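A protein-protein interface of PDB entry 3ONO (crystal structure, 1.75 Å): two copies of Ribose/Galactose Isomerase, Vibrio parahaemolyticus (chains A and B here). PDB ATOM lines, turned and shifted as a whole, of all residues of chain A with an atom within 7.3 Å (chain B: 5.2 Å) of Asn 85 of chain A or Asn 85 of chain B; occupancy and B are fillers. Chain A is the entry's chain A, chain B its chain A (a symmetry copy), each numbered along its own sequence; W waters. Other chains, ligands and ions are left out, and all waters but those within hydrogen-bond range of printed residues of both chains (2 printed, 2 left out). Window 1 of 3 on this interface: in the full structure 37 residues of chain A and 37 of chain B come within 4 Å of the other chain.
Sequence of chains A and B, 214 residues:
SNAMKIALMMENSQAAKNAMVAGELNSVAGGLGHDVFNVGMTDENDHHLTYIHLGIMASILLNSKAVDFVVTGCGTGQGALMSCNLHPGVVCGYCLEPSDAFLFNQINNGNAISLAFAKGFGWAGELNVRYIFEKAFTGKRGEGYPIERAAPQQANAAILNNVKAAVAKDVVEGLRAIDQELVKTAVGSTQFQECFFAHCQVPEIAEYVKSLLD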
ATOM      1  N   GLY A  55      16.514  13.788   8.875  1.00  0.00           N
ATOM      2  CA  GLY A  55      17.320  12.605   8.629  1.00  0.00           C
ATOM      3  C   GLY A  55      16.494  11.332   8.743  1.00  0.00           C
ATOM      4  O   GLY A  55      16.649  10.387   7.952  1.00  0.00           O
ATOM      5  N   GLN A  78      24.510  22.125   7.336  1.00  0.00           N
ATOM      6  CA  GLN A  78      25.333  21.200   8.133  1.00  0.00           C
ATOM      7  C   GLN A  78      24.512  20.225   8.984  1.00  0.00           C
ATOM      8  O   GLN A  78      24.745  19.017   8.942  1.00  0.00           O
ATOM      9  CB  GLN A  78      26.294  21.968   9.046  1.00  0.00           C
ATOM     10  CG  GLN A  78      27.243  22.937   8.294  1.00  0.00           C
ATOM     11  CD  GLN A  78      28.563  22.278   7.927  1.00  0.00           C
ATOM     12  OE1 GLN A  78      28.594  21.085   7.595  1.00  0.00           O
ATOM     13  NE2 GLN A  78      29.660  23.059   7.947  1.00  0.00           N
ATOM     14  N   GLY A  79      23.572  20.739   9.773  1.00  0.00           N
ATOM     15  CA  GLY A  79      22.768  19.857  10.614  1.00  0.00           C
ATOM     16  C   GLY A  79      22.050  18.821   9.767  1.00  0.00           C
ATOM     17  O   GLY A  79      22.053  17.623  10.066  1.00  0.00           O
ATOM     18  N   ALA A  80      21.420  19.271   8.686  1.00  0.00           N
ATOM     19  CA  ALA A  80      20.647  18.330   7.875  1.00  0.00           C
ATOM     20  C   ALA A  80      21.560  17.282   7.225  1.00  0.00           C
ATOM     21  O   ALA A  80      21.213  16.117   7.141  1.00  0.00           O
ATOM     22  CB  ALA A  80      19.829  19.077   6.812  1.00  0.00           C
ATOM     23  N   LEU A  81      22.731  17.707   6.771  1.00  0.00           N
ATOM     24  CA  LEU A  81      23.680  16.799   6.124  1.00  0.00           C
ATOM     25  C   LEU A  81      24.180  15.739   7.103  1.00  0.00           C
ATOM     26  O   LEU A  81      24.276  14.537   6.775  1.00  0.00           O
ATOM     27  CB  LEU A  81      24.841  17.647   5.597  1.00  0.00           C
ATOM     28  CG  LEU A  81      26.253  17.195   5.269  1.00  0.00           C
ATOM     29  CD1 LEU A  81      26.979  18.438   4.802  1.00  0.00           C
ATOM     30  CD2 LEU A  81      26.988  16.594   6.440  1.00  0.00           C
ATOM     31  N   MET A  82      24.484  16.165   8.325  1.00  0.00           N
ATOM     32  CA  MET A  82      25.024  15.214   9.305  1.00  0.00           C
ATOM     33  C   MET A  82      23.926  14.298   9.846  1.00  0.00           C
ATOM     34  O   MET A  82      24.169  13.107  10.127  1.00  0.00           O
ATOM     35  CB  MET A  82      25.749  15.961  10.410  1.00  0.00           C
ATOM     36  CG  MET A  82      26.945  16.741   9.849  1.00  0.00           C
ATOM     37  SD  MET A  82      27.954  17.601  11.254  1.00  0.00           S
ATOM     38  CE  MET A  82      26.475  18.600  12.018  1.00  0.00           C
ATOM     39  N   SER A  83      22.717  14.850   9.945  1.00  0.00           N
ATOM     40  CA  SER A  83      21.528  14.087  10.384  1.00  0.00           C
ATOM     41  C   SER A  83      21.141  13.017   9.362  1.00  0.00           C
ATOM     42  O   SER A  83      20.757  11.908   9.725  1.00  0.00           O
ATOM     43  CB  SER A  83      20.352  15.065  10.601  1.00  0.00           C
ATOM     44  OG  SER A  83      19.138  14.370  10.896  1.00  0.00           O
ATOM     45  N   CYS A  84      21.254  13.329   8.076  1.00  0.00           N
ATOM     46  CA  CYS A  84      20.972  12.317   7.032  1.00  0.00           C
ATOM     47  C   CYS A  84      22.044  11.228   6.984  1.00  0.00           C
ATOM     48  O   CYS A  84      21.734  10.028   6.890  1.00  0.00           O
ATOM     49  CB  CYS A  84      20.896  12.992   5.660  1.00  0.00           C
ATOM     50  SG  CYS A  84      19.358  13.908   5.412  1.00  0.00           S
ATOM     51  N   ASN A  85      23.309  11.638   6.998  1.00  0.00           N
ATOM     52  CA  ASN A  85      24.397  10.678   6.762  1.00  0.00           C
ATOM     53  C   ASN A  85      24.555   9.603   7.829  1.00  0.00           C
ATOM     54  O   ASN A  85      25.117   8.533   7.559  1.00  0.00           O
ATOM     55  CB  ASN A  85      25.730  11.403   6.529  1.00  0.00           C
ATOM     56  CG  ASN A  85      25.903  11.846   5.060  1.00  0.00           C
ATOM     57  OD1 ASN A  85      25.945  10.999   4.169  1.00  0.00           O
ATOM     58  ND2 ASN A  85      25.989  13.153   4.811  1.00  0.00           N
ATOM     59  N   LEU A  86      24.046   9.840   9.036  1.00  0.00           N
ATOM     60  CA  LEU A  86      24.142   8.790  10.055  1.00  0.00           C
ATOM     61  C   LEU A  86      23.328   7.562   9.680  1.00  0.00           C
ATOM     62  O   LEU A  86      23.632   6.456  10.116  1.00  0.00           O
ATOM     63  CB  LEU A  86      23.688   9.293  11.437  1.00  0.00           C
ATOM     64  CG  LEU A  86      22.194   9.586  11.594  1.00  0.00           C
ATOM     65  CD1 LEU A  86      21.456   8.358  12.177  1.00  0.00           C
ATOM     66  CD2 LEU A  86      21.995  10.798  12.522  1.00  0.00           C
ATOM     67  N   HIS A  87      22.288   7.740   8.875  1.00  0.00           N
ATOM     68  CA  HIS A  87      21.384   6.614   8.592  1.00  0.00           C
ATOM     69  C   HIS A  87      21.907   5.703   7.498  1.00  0.00           C
ATOM     70  O   HIS A  87      22.352   6.175   6.459  1.00  0.00           O
ATOM     71  CB  HIS A  87      20.005   7.132   8.180  1.00  0.00           C
ATOM     72  CG  HIS A  87      19.314   7.913   9.255  1.00  0.00           C
ATOM     73  ND1 HIS A  87      18.560   7.312  10.249  1.00  0.00           N
ATOM     74  CD2 HIS A  87      19.262   9.246   9.491  1.00  0.00           C
ATOM     75  CE1 HIS A  87      18.079   8.251  11.050  1.00  0.00           C
ATOM     76  NE2 HIS A  87      18.498   9.432  10.614  1.00  0.00           N
ATOM     77  N   PRO A  88      21.834   4.385   7.718  1.00  0.00           N
ATOM     78  CA  PRO A  88      22.222   3.514   6.601  1.00  0.00           C
ATOM     79  C   PRO A  88      21.319   3.769   5.404  1.00  0.00           C
ATOM     80  O   PRO A  88      20.123   4.090   5.550  1.00  0.00           O
ATOM     81  CB  PRO A  88      21.994   2.086   7.168  1.00  0.00           C
ATOM     82  CG  PRO A  88      20.923   2.273   8.248  1.00  0.00           C
ATOM     83  CD  PRO A  88      21.195   3.669   8.837  1.00  0.00           C
ATOM     84  N   GLY A  89      21.876   3.611   4.208  1.00  0.00           N
ATOM     85  CA  GLY A  89      21.094   3.783   3.007  1.00  0.00           C
ATOM     86  C   GLY A  89      20.886   5.235   2.591  1.00  0.00           C
ATOM     87  O   GLY A  89      20.246   5.490   1.574  1.00  0.00           O
ATOM     88  N   VAL A  90      21.399   6.178   3.383  1.00  0.00           N
ATOM     89  CA  VAL A  90      21.271   7.606   3.068  1.00  0.00           C
ATOM     90  C   VAL A  90      22.646   8.203   2.869  1.00  0.00           C
ATOM     91  O   VAL A  90      23.421   8.300   3.819  1.00  0.00           O
ATOM     92  CB  VAL A  90      20.568   8.368   4.208  1.00  0.00           C
ATOM     93  CG1 VAL A  90      20.359   9.840   3.810  1.00  0.00           C
ATOM     94  CG2 VAL A  90      19.226   7.681   4.535  1.00  0.00           C
ATOM     95  N   VAL A  91      22.923   8.643   1.639  1.00  0.00           N
ATOM     96  CA  VAL A  91      24.223   9.144   1.252  1.00  0.00           C
ATOM     97  C   VAL A  91      24.007  10.589   0.783  1.00  0.00           C
ATOM     98  O   VAL A  91      23.581  10.822  -0.338  1.00  0.00           O
ATOM     99  CB  VAL A  91      24.822   8.261   0.139  1.00  0.00           C
ATOM    100  CG1 VAL A  91      26.145   8.851  -0.344  1.00  0.00           C
ATOM    101  CG2 VAL A  91      25.031   6.826   0.656  1.00  0.00           C
ATOM    102  N   CYS A  92      24.272  11.551   1.672  1.00  0.00           N
ATOM    103  CA  CYS A  92      23.893  12.954   1.470  1.00  0.00           C
ATOM    104  C   CYS A  92      25.114  13.852   1.311  1.00  0.00           C
ATOM    105  O   CYS A  92      25.956  13.924   2.208  1.00  0.00           O
ATOM    106  CB  CYS A  92      23.065  13.437   2.683  1.00  0.00           C
ATOM    107  SG  CYS A  92      22.341  15.096   2.461  1.00  0.00           S
ATOM    108  N   GLY A  93      25.223  14.536   0.169  1.00  0.00           N
ATOM    109  CA  GLY A  93      26.318  15.489  -0.022  1.00  0.00           C
ATOM    110  C   GLY A  93      25.903  16.929   0.299  1.00  0.00           C
ATOM    111  O   GLY A  93      24.721  17.226   0.371  1.00  0.00           O
ATOM    112  N   TYR A  94      26.863  17.832   0.475  1.00  0.00           N
ATOM    113  CA  TYR A  94      26.520  19.256   0.515  1.00  0.00           C
ATOM    114  C   TYR A  94      26.283  19.733  -0.917  1.00  0.00           C
ATOM    115  O   TYR A  94      26.767  19.131  -1.870  1.00  0.00           O
ATOM    116  CB  TYR A  94      27.631  20.096   1.193  1.00  0.00           C
ATOM    117  CG  TYR A  94      28.936  20.187   0.422  1.00  0.00           C
ATOM    118  CD1 TYR A  94      29.060  21.048  -0.677  1.00  0.00           C
ATOM    119  CD2 TYR A  94      30.050  19.425   0.783  1.00  0.00           C
ATOM    120  CE1 TYR A  94      30.257  21.136  -1.416  1.00  0.00           C
ATOM    121  CE2 TYR A  94      31.264  19.519   0.055  1.00  0.00           C
ATOM    122  CZ  TYR A  94      31.351  20.372  -1.034  1.00  0.00           C
ATOM    123  OH  TYR A  94      32.519  20.451  -1.763  1.00  0.00           O
ATOM    124  N   PHE A 104      28.855  15.691  -7.377  1.00  0.00           N
ATOM    125  CA  PHE A 104      28.290  14.741  -6.425  1.00  0.00           C
ATOM    126  C   PHE A 104      27.685  13.549  -7.167  1.00  0.00           C
ATOM    127  O   PHE A 104      27.947  12.394  -6.832  1.00  0.00           O
ATOM    128  CB  PHE A 104      27.222  15.409  -5.565  1.00  0.00           C
ATOM    129  CG  PHE A 104      26.524  14.464  -4.603  1.00  0.00           C
ATOM    130  CD1 PHE A 104      27.170  13.990  -3.475  1.00  0.00           C
ATOM    131  CD2 PHE A 104      25.211  14.075  -4.833  1.00  0.00           C
ATOM    132  CE1 PHE A 104      26.513  13.152  -2.583  1.00  0.00           C
ATOM    133  CE2 PHE A 104      24.552  13.223  -3.938  1.00  0.00           C
ATOM    134  CZ  PHE A 104      25.217  12.770  -2.820  1.00  0.00           C
ATOM    135  N   ASN A 111      22.256   9.811  -2.847  1.00  0.00           N
ATOM    136  CA  ASN A 111      20.807   9.930  -3.024  1.00  0.00           C
ATOM    137  C   ASN A 111      20.173  11.069  -2.223  1.00  0.00           C
ATOM    138  O   ASN A 111      18.968  11.112  -2.054  1.00  0.00           O
ATOM    139  CB  ASN A 111      20.092   8.585  -2.714  1.00  0.00           C
ATOM    140  CG  ASN A 111      20.381   8.065  -1.325  1.00  0.00           C
ATOM    141  OD1 ASN A 111      21.007   8.743  -0.505  1.00  0.00           O
ATOM    142  ND2 ASN A 111      19.924   6.833  -1.046  1.00  0.00           N
ATOM    143  N   ALA A 112      20.987  11.996  -1.739  1.00  0.00           N
ATOM    144  CA  ALA A 112      20.446  13.169  -1.057  1.00  0.00           C
ATOM    145  C   ALA A 112      21.419  14.321  -1.174  1.00  0.00           C
ATOM    146  O   ALA A 112      22.620  14.096  -1.263  1.00  0.00           O
ATOM    147  CB  ALA A 112      20.187  12.851   0.400  1.00  0.00           C
ATOM    148  N   SER A 114      22.122  18.390   0.580  1.00  0.00           N
ATOM    149  CA  SER A 114      21.730  19.356   1.612  1.00  0.00           C
ATOM    150  C   SER A 114      22.192  20.743   1.212  1.00  0.00           C
ATOM    151  O   SER A 114      23.390  20.979   1.019  1.00  0.00           O
ATOM    152  CB  SER A 114      22.343  18.980   2.953  1.00  0.00           C
ATOM    153  OG  SER A 114      21.984  19.917   3.970  1.00  0.00           O
ATOM    154  N   LEU A 160      31.416   2.540   0.536  1.00  0.00           N
ATOM    155  CA  LEU A 160      30.771   3.417   1.509  1.00  0.00           C
ATOM    156  C   LEU A 160      29.444   2.796   1.948  1.00  0.00           C
ATOM    157  O   LEU A 160      29.115   2.796   3.126  1.00  0.00           O
ATOM    158  CB  LEU A 160      30.541   4.838   0.942  1.00  0.00           C
ATOM    159  CG  LEU A 160      29.822   5.808   1.888  1.00  0.00           C
ATOM    160  CD1 LEU A 160      30.689   6.083   3.121  1.00  0.00           C
ATOM    161  CD2 LEU A 160      29.503   7.104   1.169  1.00  0.00           C
ATOM    162  N   LYS A 164      28.473   1.668   5.815  1.00  0.00           N
ATOM    163  CA  LYS A 164      27.285   2.215   6.469  1.00  0.00           C
ATOM    164  C   LYS A 164      26.399   1.077   6.969  1.00  0.00           C
ATOM    165  O   LYS A 164      25.923   1.100   8.090  1.00  0.00           O
ATOM    166  CB  LYS A 164      26.498   3.108   5.508  1.00  0.00           C
ATOM    167  CG  LYS A 164      27.237   4.427   5.159  1.00  0.00           C
ATOM    168  CD  LYS A 164      26.552   5.258   4.028  1.00  0.00           C
ATOM    169  CE  LYS A 164      25.127   5.715   4.379  1.00  0.00           C
ATOM    170  NZ  LYS A 164      25.057   6.717   5.521  1.00  0.00           N
ATOM    171  N   ALA B  80      34.891  12.137   2.142  1.00  0.00           N
ATOM    172  CA  ALA B  80      35.414  12.095   3.508  1.00  0.00           C
ATOM    173  C   ALA B  80      34.335  12.495   4.523  1.00  0.00           C
ATOM    174  O   ALA B  80      34.237  11.916   5.592  1.00  0.00           O
ATOM    175  CB  ALA B  80      36.652  12.992   3.643  1.00  0.00           C
ATOM    176  N   LEU B  81      33.526  13.486   4.178  1.00  0.00           N
ATOM    177  CA  LEU B  81      32.466  13.960   5.070  1.00  0.00           C
ATOM    178  C   LEU B  81      31.418  12.875   5.302  1.00  0.00           C
ATOM    179  O   LEU B  81      30.956  12.642   6.439  1.00  0.00           O
ATOM    180  CB  LEU B  81      31.837  15.196   4.421  1.00  0.00           C
ATOM    181  CG  LEU B  81      30.460  15.784   4.673  1.00  0.00           C
ATOM    182  CD1 LEU B  81      30.358  16.986   3.759  1.00  0.00           C
ATOM    183  CD2 LEU B  81      29.329  14.832   4.378  1.00  0.00           C
ATOM    184  N   MET B  82      31.045  12.179   4.232  1.00  0.00           N
ATOM    185  CA  MET B  82      30.000  11.156   4.366  1.00  0.00           C
ATOM    186  C   MET B  82      30.544   9.901   5.051  1.00  0.00           C
ATOM    187  O   MET B  82      29.826   9.231   5.819  1.00  0.00           O
ATOM    188  CB  MET B  82      29.389  10.855   3.009  1.00  0.00           C
ATOM    189  CG  MET B  82      28.711  12.101   2.427  1.00  0.00           C
ATOM    190  SD  MET B  82      27.823  11.711   0.757  1.00  0.00           S
ATOM    191  CE  MET B  82      29.371  10.987  -0.162  1.00  0.00           C
ATOM    192  N   SER B  83      31.822   9.620   4.799  1.00  0.00           N
ATOM    193  CA  SER B  83      32.526   8.483   5.431  1.00  0.00           C
ATOM    194  C   SER B  83      32.695   8.697   6.936  1.00  0.00           C
ATOM    195  O   SER B  83      32.557   7.765   7.726  1.00  0.00           O
ATOM    196  CB  SER B  83      33.907   8.307   4.761  1.00  0.00           C
ATOM    197  OG  SER B  83      34.688   7.309   5.422  1.00  0.00           O
ATOM    198  N   CYS B  84      32.975   9.927   7.352  1.00  0.00           N
ATOM    199  CA  CYS B  84      33.075  10.223   8.800  1.00  0.00           C
ATOM    200  C   CYS B  84      31.712  10.174   9.491  1.00  0.00           C
ATOM    201  O   CYS B  84      31.569   9.601  10.586  1.00  0.00           O
ATOM    202  CB  CYS B  84      33.678  11.615   9.006  1.00  0.00           C
ATOM    203  SG  CYS B  84      35.461  11.657   8.713  1.00  0.00           S
ATOM    204  N   ASN B  85      30.715  10.811   8.886  1.00  0.00           N
ATOM    205  CA  ASN B  85      29.423  10.978   9.569  1.00  0.00           C
ATOM    206  C   ASN B  85      28.661   9.687   9.837  1.00  0.00           C
ATOM    207  O   ASN B  85      27.814   9.638  10.739  1.00  0.00           O
ATOM    208  CB  ASN B  85      28.533  11.983   8.826  1.00  0.00           C
ATOM    209  CG  ASN B  85      28.846  13.443   9.221  1.00  0.00           C
ATOM    210  OD1 ASN B  85      28.680  13.808  10.384  1.00  0.00           O
ATOM    211  ND2 ASN B  85      29.302  14.260   8.272  1.00  0.00           N
ATOM    212  N   LEU B  86      28.959   8.620   9.098  1.00  0.00           N
ATOM    213  CA  LEU B  86      28.272   7.357   9.385  1.00  0.00           C
ATOM    214  C   LEU B  86      28.633   6.816  10.758  1.00  0.00           C
ATOM    215  O   LEU B  86      27.859   6.079  11.362  1.00  0.00           O
ATOM    216  CB  LEU B  86      28.580   6.287   8.323  1.00  0.00           C
ATOM    217  CG  LEU B  86      30.009   5.737   8.311  1.00  0.00           C
ATOM    218  CD1 LEU B  86      30.103   4.442   9.151  1.00  0.00           C
ATOM    219  CD2 LEU B  86      30.444   5.447   6.863  1.00  0.00           C
ATOM    220  N   HIS B  87      29.809   7.167  11.265  1.00  0.00           N
ATOM    221  CA  HIS B  87      30.271   6.562  12.524  1.00  0.00           C
ATOM    222  C   HIS B  87      29.689   7.242  13.748  1.00  0.00           C
ATOM    223  O   HIS B  87      29.676   8.465  13.831  1.00  0.00           O
ATOM    224  CB  HIS B  87      31.797   6.620  12.611  1.00  0.00           C
ATOM    225  CG  HIS B  87      32.487   5.836  11.538  1.00  0.00           C
ATOM    226  ND1 HIS B  87      32.741   4.480  11.648  1.00  0.00           N
ATOM    227  CD2 HIS B  87      32.977   6.219  10.334  1.00  0.00           C
ATOM    228  CE1 HIS B  87      33.356   4.067  10.551  1.00  0.00           C
ATOM    229  NE2 HIS B  87      33.504   5.104   9.735  1.00  0.00           N
ATOM    230  N   VAL B  90      31.182  10.623  15.687  1.00  0.00           N
ATOM    231  CA  VAL B  90      31.891  11.468  14.720  1.00  0.00           C
ATOM    232  C   VAL B  90      30.907  12.404  14.053  1.00  0.00           C
ATOM    233  O   VAL B  90      30.043  11.959  13.301  1.00  0.00           O
ATOM    234  CB  VAL B  90      32.570  10.618  13.629  1.00  0.00           C
ATOM    235  CG1 VAL B  90      33.387  11.522  12.687  1.00  0.00           C
ATOM    236  CG2 VAL B  90      33.465   9.550  14.293  1.00  0.00           C
ATOM    237  N   VAL B  91      31.075  13.706  14.301  1.00  0.00           N
ATOM    238  CA  VAL B  91      30.163  14.725  13.831  1.00  0.00           C
ATOM    239  C   VAL B  91      30.990  15.672  12.950  1.00  0.00           C
ATOM    240  O   VAL B  91      31.696  16.532  13.454  1.00  0.00           O
ATOM    241  CB  VAL B  91      29.527  15.460  15.026  1.00  0.00           C
ATOM    242  CG1 VAL B  91      28.647  16.606  14.531  1.00  0.00           C
ATOM    243  CG2 VAL B  91      28.699  14.477  15.875  1.00  0.00           C
ATOM    244  N   CYS B  92      30.920  15.472  11.630  1.00  0.00           N
ATOM    245  CA  CYS B  92      31.823  16.122  10.674  1.00  0.00           C
ATOM    246  C   CYS B  92      31.082  17.102   9.773  1.00  0.00           C
ATOM    247  O   CYS B  92      30.159  16.714   9.054  1.00  0.00           O
ATOM    248  CB  CYS B  92      32.499  15.043   9.798  1.00  0.00           C
ATOM    249  SG  CYS B  92      33.813  15.695   8.715  1.00  0.00           S
ATOM    250  N   GLY B  93      31.474  18.379   9.809  1.00  0.00           N
ATOM    251  CA  GLY B  93      30.873  19.363   8.906  1.00  0.00           C
ATOM    252  C   GLY B  93      31.714  19.590   7.646  1.00  0.00           C
ATOM    253  O   GLY B  93      32.880  19.227   7.610  1.00  0.00           O
ATOM    254  N   LYS B 164      22.603   9.242  16.580  1.00  0.00           N
ATOM    255  CA  LYS B 164      23.745   8.514  16.028  1.00  0.00           C
ATOM    256  C   LYS B 164      24.023   7.272  16.872  1.00  0.00           C
ATOM    257  O   LYS B 164      24.228   6.192  16.347  1.00  0.00           O
ATOM    258  CB  LYS B 164      24.988   9.405  15.983  1.00  0.00           C
ATOM    259  CG  LYS B 164      24.878  10.549  14.941  1.00  0.00           C
ATOM    260  CD  LYS B 164      26.040  11.589  15.016  1.00  0.00           C
ATOM    261  CE  LYS B 164      27.426  10.981  14.751  1.00  0.00           C
ATOM    262  NZ  LYS B 164      27.622  10.470  13.332  1.00  0.00           N
HETATM  263  O   HOH W   1      26.505  12.683  11.828  1.00  0.00           O
HETATM  264  O   HOH W   2      27.199   8.518   4.760  1.00  0.00           O
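The side-chain sulfur (SD) of Met 82 of chain A lies close to the backbone NH (N) of Cys 92 of chain B. N of Cys 92 of chain A sits close to SD of Met 82 of chain B (3.7 Å).
ND2 of Asn 85 of chain A sits at hydrogen-bond distance from O of Cys 92 of chain A (2.7 Å). The backbone carbonyl oxygen (O) of Asn 85 of chain A is in hydrogen-bond range of the side-chain amino group (NZ) of Lys 164 of chain A (2.7 Å). NZ of Lys 164 of chain A is in hydrogen-bond range of O of His 87 of chain A, 2.9 Å away. The backbone carbonyl oxygen (O) of Val 90 of chain A sits at hydrogen-bond distance from the side-chain amino group (NZ) of Lys 164 of chain A, at 2.8 Å. The backbone carbonyl oxygen (O) of Ala 112 of chain A sits at hydrogen-bond distance from the backbone NH (N) of Gly 93 of chain A. The backbone carbonyl oxygen (O) of Ser 83 of chain B lies close to a ring nitrogen (NE2) of His 87 of chain B.
Among the printed residues, merely in contact across the chains: Gln 78 of chain A with Gly 93 of chain B (3.1 Å), Met 82 of chain A with Asn 85 of chain B (3.4 Å), Asn 85 of chain A with Met 82 of chain B (3.4 Å), Val 91 of chain A with Met 82 of chain B (3.5 Å), Met 82 of chain A with Val 91 of chain B (3.5 Å), Leu 81 of chain A with Leu 81 of chain B (3.6 Å), Asn 85 of chain A with Asn 85 of chain B (3.7 Å), Leu 81 of chain A with Asn 85 of chain B (3.8 Å), Asn 85 of chain A with Leu 81 of chain B (3.8 Å), Leu 86 of chain A with Lys 164 of chain B (3.8 Å), Lys 164 of chain A with Leu 86 of chain B (3.8 Å), Leu 160 of chain A with Leu 86 of chain B (3.8 Å), Leu 160 of chain A with Ser 83 of chain B (3.8 Å), Leu 86 of chain A with Asn 85 of chain B (3.8 Å), Asn 85 of chain A with Leu 86 of chain B (3.8 Å), Tyr 94 of chain A with Leu 81 of chain B (3.9 Å), Phe 104 of chain A with Met 82 of chain B (3.9 Å), Met 82 of chain A with Gly 93 of chain B (3.9 Å) and Gly 93 of chain A with Met 82 of chain B (3.9 Å).
Cys 84 of chain A touches none of the printed residues of chain B. Printed residues of chain B within 4 Å of Leu 86 of chain A: Asn 85 (3.8 Å) and Lys 164 (3.8 Å). Printed residues of chain B within 4 Å of Val 91 of chain A: Met 82. Of the printed residues of chain B, Leu 160 of chain A touches Ser 83 and Leu 86. Printed residues of chain A within 4 Å of Asn 85 of chain B: Leu 81, Met 82, Asn 85 and Leu 86. Printed residues of chain A within 4 Å of Gly 93 of chain B: Gln 78 (3.1 Å) and Met 82 (3.9 Å). The nearest printed residue of chain A that does not touch Asn 85 of chain B is Ser 83 of chain A (6.1 Å). The nearest printed residue of chain B that does not touch Gln 78 of chain A is Cys 92 of chain B (4.9 Å).
Hydrophobic or aromatic side chains of chain A within 4 Å of the printed part of chain B: Leu 81, Met 82, Leu 86, Val 91, Tyr 94, Phe 104 and Leu 160. Of the 13 printed residues of chain B, 9 touch a printed residue of chain A. Printed residues of chain B that touch a printed residue of chain A: Leu 81, Met 82, Ser 83, Asn 85, Leu 86, Val 91, Cys 92, Gly 93 and Lys 164. Hydrophobic or aromatic side chains of chain B within 4 Å of the printed part of chain A: Leu 81, Met 82, Leu 86 and Val 91. Among the printed residues, 21 pairs touch across the chains. Among the printed residues, no Asp or Glu carboxylate lies within 4 Å of a Lys or Arg side-chain nitrogen of the other chain.
Leu 81 of chain B touches its own counterpart, Leu 81 of chain A. Leu 81 of chain A touches Asn 85 of chain B, and with the chains exchanged Asn 85 of chain A touches Leu 81 of chain B. Met 82 of chain A touches Asn 85 of chain B, and with the chains exchanged Asn 85 of chain A touches Met 82 of chain B. Met 82 of chain A touches Cys 92 of chain B, and with the chains exchanged Cys 92 of chain A touches Met 82 of chain B. Of the 21 pairs that touch across the chains among the printed residues, 16 have their exchanged pair printed and touching as well.
Water W1 lies within hydrogen-bond range of OD1 of Asn 85 of chain B, NZ of Lys 164 of chain B and O of Met 82 of chain A. Water W2 lies within hydrogen-bond range of the side-chain amide oxygen (OD1) of Asn 85 of chain A (2.8 Å), the side-chain amino group (NZ) of Lys 164 of chain A (2.9 Å) and the backbone carbonyl oxygen (O) of Met 82 of chain B (2.9 Å).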
